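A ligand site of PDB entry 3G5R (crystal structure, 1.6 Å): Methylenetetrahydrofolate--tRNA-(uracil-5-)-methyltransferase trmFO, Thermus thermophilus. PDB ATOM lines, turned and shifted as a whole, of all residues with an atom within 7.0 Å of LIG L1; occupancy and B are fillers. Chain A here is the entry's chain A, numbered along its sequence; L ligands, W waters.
A nitrogen (N4) of LIG L1 sits at hydrogen-bond distance from a nitrogen (N8) of LG2 L2 (3.4 Å).
Water W2 lies within hydrogen-bond range of an oxygen (O1) of LIG L1 (2.6 Å) and a nitrogen (N7) of LG2 L2 (3.4 Å).
Water W3 lies within hydrogen-bond range of the backbone carbonyl oxygen of Arg 309 (2.8 Å) and a nitrogen (N2) of LIG L1 (2.8 Å).
Water W1 lies within hydrogen-bond range of N1 of LIG L1 (3.0 Å) and OD1 of Asn 310 (3.2 Å).
Merely in contact with LIG L1: His 308 (3.4 Å), Pro 135 (3.6 Å) and Glu 341 (3.9 Å).
Hydrophobic or aromatic side chains that line LIG L1: Pro 135 and His 308.
The nearest printed residue that does not touch LIG L1 is Cys 51 (4.8 Å).
The guanidinium group (NH1) of Arg 309 lies within hydrogen-bond range of the backbone carbonyl oxygen (O) of Pro 135, at 3.5 Å.
OG1 of Thr 311 is in hydrogen-bond range of NH1 of Arg 309, 2.8 Å away.
OD2 of Asp 158 sits at hydrogen-bond distance from N of His 308 (2.8 Å).
N of Thr 311 lies within hydrogen-bond range of O of Pro 135 (2.9 Å).
A nitrogen (N5) of LIG L1 lies within hydrogen-bond range of the side-chain amide oxygen (OD1) of Asn 310, 2.7 Å away.
N5 of LIG L1 lies within hydrogen-bond range of O of Arg 309 (2.9 Å).
The backbone NH of Gly 342 lies close to an oxygen (O9) of LG2 L2.
The backbone carbonyl oxygen of Gly 342 sits close to an oxygen (O9) of LG2 L2, 3.4 Å away.
An oxygen (O13) of LG2 L2 lies within hydrogen-bond range of the backbone NH (N) of Val 336 (2.9 Å).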
ATOM      1  N   CYS A  51     -18.716 -11.480 -14.423  1.00  0.00           N
ATOM      2  CA  CYS A  51     -19.544 -12.228 -15.357  1.00  0.00           C
ATOM      3  C   CYS A  51     -19.871 -11.431 -16.619  1.00  0.00           C
ATOM      4  O   CYS A  51     -18.981 -11.110 -17.400  1.00  0.00           O
ATOM      5  CB  CYS A  51     -20.819 -12.716 -14.671  1.00  0.00           C
ATOM      6  SG  CYS A  51     -21.649 -14.094 -15.516  1.00  0.00           S
ATOM      7  N   PRO A 135     -21.161 -10.293  -2.827  1.00  0.00           N
ATOM      8  CA  PRO A 135     -21.905 -11.556  -2.693  1.00  0.00           C
ATOM      9  C   PRO A 135     -21.029 -12.655  -2.101  1.00  0.00           C
ATOM     10  O   PRO A 135     -21.538 -13.604  -1.502  1.00  0.00           O
ATOM     11  CB  PRO A 135     -22.266 -11.894  -4.144  1.00  0.00           C
ATOM     12  CG  PRO A 135     -21.205 -11.178  -4.958  1.00  0.00           C
ATOM     13  CD  PRO A 135     -21.067  -9.874  -4.240  1.00  0.00           C
ATOM     14  N   LEU A 136     -19.712 -12.520  -2.258  1.00  0.00           N
ATOM     15  CA  LEU A 136     -18.785 -13.524  -1.755  1.00  0.00           C
ATOM     16  C   LEU A 136     -17.916 -12.950  -0.623  1.00  0.00           C
ATOM     17  O   LEU A 136     -16.729 -13.244  -0.531  1.00  0.00           O
ATOM     18  CB  LEU A 136     -17.931 -14.072  -2.896  1.00  0.00           C
ATOM     19  CG  LEU A 136     -18.756 -14.726  -4.013  1.00  0.00           C
ATOM     20  CD1 LEU A 136     -17.878 -15.110  -5.198  1.00  0.00           C
ATOM     21  CD2 LEU A 136     -19.518 -15.925  -3.471  1.00  0.00           C
ATOM     22  N   ASP A 158     -29.712 -15.930  -1.839  1.00  0.00           N
ATOM     23  CA  ASP A 158     -31.032 -15.366  -2.075  1.00  0.00           C
ATOM     24  C   ASP A 158     -31.922 -16.417  -2.735  1.00  0.00           C
ATOM     25  O   ASP A 158     -31.437 -17.379  -3.327  1.00  0.00           O
ATOM     26  CB  ASP A 158     -30.986 -14.029  -2.848  1.00  0.00           C
ATOM     27  CG  ASP A 158     -30.240 -14.109  -4.160  1.00  0.00           C
ATOM     28  OD1 ASP A 158     -29.817 -13.035  -4.658  1.00  0.00           O
ATOM     29  OD2 ASP A 158     -30.088 -15.202  -4.730  1.00  0.00           O
ATOM     30  N   VAL A 306     -34.729 -15.193  -8.720  1.00  0.00           N
ATOM     31  CA  VAL A 306     -33.382 -15.744  -8.825  1.00  0.00           C
ATOM     32  C   VAL A 306     -33.051 -16.581  -7.599  1.00  0.00           C
ATOM     33  O   VAL A 306     -33.653 -16.422  -6.540  1.00  0.00           O
ATOM     34  CB  VAL A 306     -32.302 -14.648  -8.952  1.00  0.00           C
ATOM     35  CG1 VAL A 306     -32.487 -13.848 -10.246  1.00  0.00           C
ATOM     36  CG2 VAL A 306     -32.336 -13.732  -7.744  1.00  0.00           C
ATOM     37  N   MET A 307     -32.068 -17.452  -7.756  1.00  0.00           N
ATOM     38  CA  MET A 307     -31.560 -18.225  -6.631  1.00  0.00           C
ATOM     39  C   MET A 307     -30.050 -18.362  -6.783  1.00  0.00           C
ATOM     40  O   MET A 307     -29.566 -19.119  -7.629  1.00  0.00           O
ATOM     41  CB  MET A 307     -32.240 -19.593  -6.576  1.00  0.00           C
ATOM     42  CG  MET A 307     -33.733 -19.474  -6.301  1.00  0.00           C
ATOM     43  SD  MET A 307     -34.576 -21.048  -6.205  1.00  0.00           S
ATOM     44  CE  MET A 307     -33.649 -21.830  -4.890  1.00  0.00           C
ATOM     45  N   HIS A 308     -29.314 -17.592  -5.988  1.00  0.00           N
ATOM     46  CA  HIS A 308     -27.864 -17.498  -6.104  1.00  0.00           C
ATOM     47  C   HIS A 308     -27.181 -17.589  -4.752  1.00  0.00           C
ATOM     48  O   HIS A 308     -27.727 -17.187  -3.727  1.00  0.00           O
ATOM     49  CB  HIS A 308     -27.448 -16.149  -6.690  1.00  0.00           C
ATOM     50  CG  HIS A 308     -27.852 -15.947  -8.111  1.00  0.00           C
ATOM     51  ND1 HIS A 308     -28.358 -14.756  -8.582  1.00  0.00           N
ATOM     52  CD2 HIS A 308     -27.826 -16.787  -9.175  1.00  0.00           C
ATOM     53  CE1 HIS A 308     -28.621 -14.869  -9.865  1.00  0.00           C
ATOM     54  NE2 HIS A 308     -28.302 -16.084 -10.253  1.00  0.00           N
ATOM     55  N   ARG A 309     -25.953 -18.094  -4.767  1.00  0.00           N
ATOM     56  CA  ARG A 309     -25.030 -17.854  -3.671  1.00  0.00           C
ATOM     57  C   ARG A 309     -24.797 -16.344  -3.623  1.00  0.00           C
ATOM     58  O   ARG A 309     -24.319 -15.753  -4.589  1.00  0.00           O
ATOM     59  CB  ARG A 309     -23.730 -18.615  -3.917  1.00  0.00           C
ATOM     60  CG  ARG A 309     -22.575 -18.191  -3.029  1.00  0.00           C
ATOM     61  CD  ARG A 309     -22.653 -18.809  -1.647  1.00  0.00           C
ATOM     62  NE  ARG A 309     -21.466 -18.419  -0.885  1.00  0.00           N
ATOM     63  CZ  ARG A 309     -21.409 -17.346  -0.109  1.00  0.00           C
ATOM     64  NH1 ARG A 309     -22.481 -16.573   0.043  1.00  0.00           N
ATOM     65  NH2 ARG A 309     -20.289 -17.061   0.541  1.00  0.00           N
ATOM     66  N   ASN A 310     -25.165 -15.721  -2.509  1.00  0.00           N
ATOM     67  CA  ASN A 310     -25.212 -14.265  -2.420  1.00  0.00           C
ATOM     68  C   ASN A 310     -25.314 -13.823  -0.959  1.00  0.00           C
ATOM     69  O   ASN A 310     -26.393 -13.893  -0.367  1.00  0.00           O
ATOM     70  CB  ASN A 310     -26.433 -13.770  -3.194  1.00  0.00           C
ATOM     71  CG  ASN A 310     -26.461 -12.264  -3.378  1.00  0.00           C
ATOM     72  OD1 ASN A 310     -25.830 -11.725  -4.286  1.00  0.00           O
ATOM     73  ND2 ASN A 310     -27.238 -11.580  -2.538  1.00  0.00           N
ATOM     74  N   THR A 311     -24.202 -13.403  -0.372  1.00  0.00           N
ATOM     75  CA  THR A 311     -24.213 -12.907   0.997  1.00  0.00           C
ATOM     76  C   THR A 311     -24.781 -11.493   1.041  1.00  0.00           C
ATOM     77  O   THR A 311     -24.296 -10.605   0.334  1.00  0.00           O
ATOM     78  CB  THR A 311     -22.795 -12.929   1.594  1.00  0.00           C
ATOM     79  OG1 THR A 311     -22.362 -14.287   1.716  1.00  0.00           O
ATOM     80  CG2 THR A 311     -22.773 -12.263   2.958  1.00  0.00           C
ATOM     81  N   VAL A 336     -23.851  -5.409  -2.997  1.00  0.00           N
ATOM     82  CA  VAL A 336     -24.638  -6.609  -2.719  1.00  0.00           C
ATOM     83  C   VAL A 336     -24.822  -6.830  -1.217  1.00  0.00           C
ATOM     84  O   VAL A 336     -25.899  -7.238  -0.775  1.00  0.00           O
ATOM     85  CB  VAL A 336     -23.978  -7.831  -3.367  1.00  0.00           C
ATOM     86  CG1 VAL A 336     -24.510  -9.118  -2.756  1.00  0.00           C
ATOM     87  CG2 VAL A 336     -24.217  -7.814  -4.886  1.00  0.00           C
ATOM     88  N   GLU A 341     -28.620  -5.739  -6.194  1.00  0.00           N
ATOM     89  CA  GLU A 341     -28.095  -6.651  -7.178  1.00  0.00           C
ATOM     90  C   GLU A 341     -27.788  -5.836  -8.437  1.00  0.00           C
ATOM     91  O   GLU A 341     -28.593  -4.994  -8.843  1.00  0.00           O
ATOM     92  CB  GLU A 341     -29.133  -7.738  -7.488  1.00  0.00           C
ATOM     93  CG  GLU A 341     -28.840  -8.635  -8.683  1.00  0.00           C
ATOM     94  CD  GLU A 341     -29.926  -9.666  -8.930  1.00  0.00           C
ATOM     95  OE1 GLU A 341     -30.442 -10.255  -7.946  1.00  0.00           O
ATOM     96  OE2 GLU A 341     -30.269  -9.916 -10.109  1.00  0.00           O
ATOM     97  N   GLY A 342     -26.614  -6.047  -9.021  1.00  0.00           N
ATOM     98  CA  GLY A 342     -26.229  -5.391 -10.258  1.00  0.00           C
ATOM     99  C   GLY A 342     -24.977  -4.560 -10.085  1.00  0.00           C
ATOM    100  O   GLY A 342     -24.799  -3.926  -9.041  1.00  0.00           O
HETATM  101  N1  LIG L   1     -25.690 -12.433  -8.212  1.00  0.00           N
HETATM  102  C1  LIG L   1     -25.080 -13.479  -7.602  1.00  0.00           C
HETATM  103  N2  LIG L   1     -24.677 -14.582  -8.339  1.00  0.00           N
HETATM  104  C2  LIG L   1     -24.875 -14.607  -9.683  1.00  0.00           C
HETATM  105  C3  LIG L   1     -25.511 -13.512 -10.337  1.00  0.00           C
HETATM  106  C4  LIG L   1     -25.898 -12.458  -9.616  1.00  0.00           C
HETATM  107  N3  LIG L   1     -24.445 -15.795 -10.494  1.00  0.00           N
HETATM  108  C5  LIG L   1     -24.398 -15.640 -11.964  1.00  0.00           C
HETATM  109  C6  LIG L   1     -25.566 -14.768 -12.453  1.00  0.00           C
HETATM  110  N4  LIG L   1     -25.694 -13.547 -11.755  1.00  0.00           N
HETATM  111  O1  LIG L   1     -26.523 -11.380 -10.238  1.00  0.00           O
HETATM  112  N5  LIG L   1     -24.844 -13.444  -6.175  1.00  0.00           N
HETATM  113  P1  LG2 L   2     -17.801  -7.234  -5.427  1.00  0.00           P
HETATM  114  O1  LG2 L   2     -17.715  -8.736  -5.401  1.00  0.00           O
HETATM  115  O2  LG2 L   2     -17.644  -6.607  -6.785  1.00  0.00           O
HETATM  116  O3  LG2 L   2     -16.675  -6.608  -4.464  1.00  0.00           O
HETATM  117  C1  LG2 L   2     -16.513  -7.064  -3.153  1.00  0.00           C
HETATM  118  C2  LG2 L   2     -15.014  -7.041  -2.883  1.00  0.00           C
HETATM  119  O4  LG2 L   2     -14.794  -7.309  -1.513  1.00  0.00           O
HETATM  120  C3  LG2 L   2     -14.271  -8.134  -3.665  1.00  0.00           C
HETATM  121  O5  LG2 L   2     -13.165  -7.550  -4.320  1.00  0.00           O
HETATM  122  C4  LG2 L   2     -13.805  -9.111  -2.599  1.00  0.00           C
HETATM  123  O6  LG2 L   2     -12.546  -9.658  -2.914  1.00  0.00           O
HETATM  124  C5  LG2 L   2     -13.703  -8.193  -1.390  1.00  0.00           C
HETATM  125  N1  LG2 L   2     -13.818  -8.837  -0.069  1.00  0.00           N
HETATM  126  C6  LG2 L   2     -14.734  -9.771   0.337  1.00  0.00           C
HETATM  127  N2  LG2 L   2     -14.495 -10.046   1.641  1.00  0.00           N
HETATM  128  C7  LG2 L   2     -13.459  -9.288   2.071  1.00  0.00           C
HETATM  129  C8  LG2 L   2     -12.799  -9.173   3.287  1.00  0.00           C
HETATM  130  N3  LG2 L   2     -13.311  -9.739   4.381  1.00  0.00           N
HETATM  131  N4  LG2 L   2     -11.749  -8.277   3.410  1.00  0.00           N
HETATM  132  C9  LG2 L   2     -11.337  -7.533   2.317  1.00  0.00           C
HETATM  133  N5  LG2 L   2     -11.987  -7.658   1.111  1.00  0.00           N
HETATM  134  C10 LG2 L   2     -13.027  -8.522   1.001  1.00  0.00           C
HETATM  135  N6  LG2 L   2     -24.132  -8.473 -11.612  1.00  0.00           N
HETATM  136  C11 LG2 L   2     -24.519  -7.945 -12.824  1.00  0.00           C
HETATM  137  O7  LG2 L   2     -25.001  -6.814 -12.885  1.00  0.00           O
HETATM  138  N7  LG2 L   2     -24.392  -8.701 -13.977  1.00  0.00           N
HETATM  139  C12 LG2 L   2     -23.850  -9.968 -13.905  1.00  0.00           C
HETATM  140  O8  LG2 L   2     -23.718 -10.634 -14.929  1.00  0.00           O
HETATM  141  C13 LG2 L   2     -23.446 -10.486 -12.678  1.00  0.00           C
HETATM  142  N8  LG2 L   2     -22.906 -11.763 -12.605  1.00  0.00           N
HETATM  143  C14 LG2 L   2     -22.505 -12.250 -11.382  1.00  0.00           C
HETATM  144  C15 LG2 L   2     -21.965 -13.526 -11.309  1.00  0.00           C
HETATM  145  C16 LG2 L   2     -21.550 -14.037 -10.085  1.00  0.00           C
HETATM  146  C17 LG2 L   2     -20.963 -15.419 -10.014  1.00  0.00           C
HETATM  147  C18 LG2 L   2     -21.696 -13.275  -8.929  1.00  0.00           C
HETATM  148  C19 LG2 L   2     -21.260 -13.820  -7.600  1.00  0.00           C
HETATM  149  C20 LG2 L   2     -22.236 -11.999  -9.003  1.00  0.00           C
HETATM  150  C21 LG2 L   2     -22.649 -11.478 -10.228  1.00  0.00           C
HETATM  151  N9  LG2 L   2     -23.209 -10.205 -10.287  1.00  0.00           N
HETATM  152  C22 LG2 L   2     -23.583  -9.727 -11.524  1.00  0.00           C
HETATM  153  C23 LG2 L   2     -23.870  -9.610  -9.072  1.00  0.00           C
HETATM  154  C24 LG2 L   2     -23.270  -8.271  -8.586  1.00  0.00           C
HETATM  155  O9  LG2 L   2     -23.767  -7.158  -9.305  1.00  0.00           O
HETATM  156  C25 LG2 L   2     -21.745  -8.286  -8.647  1.00  0.00           C
HETATM  157  O10 LG2 L   2     -21.286  -9.291  -7.762  1.00  0.00           O
HETATM  158  C26 LG2 L   2     -21.120  -6.936  -8.272  1.00  0.00           C
HETATM  159  O11 LG2 L   2     -19.735  -6.996  -8.534  1.00  0.00           O
HETATM  160  C27 LG2 L   2     -21.327  -6.624  -6.796  1.00  0.00           C
HETATM  161  O12 LG2 L   2     -20.568  -5.483  -6.424  1.00  0.00           O
HETATM  162  P2  LG2 L   2     -19.966  -5.410  -4.938  1.00  0.00           P
HETATM  163  O13 LG2 L   2     -21.121  -5.421  -3.967  1.00  0.00           O
HETATM  164  O14 LG2 L   2     -19.024  -4.240  -4.820  1.00  0.00           O
HETATM  165  O15 LG2 L   2     -19.204  -6.829  -4.764  1.00  0.00           O
HETATM  166  O   HOH W   1     -26.789 -10.013  -6.815  1.00  0.00           O
HETATM  167  O   HOH W   2     -26.826 -10.817 -12.763  1.00  0.00           O
HETATM  168  O   HOH W   3     -23.336 -16.705  -7.037  1.00  0.00           O
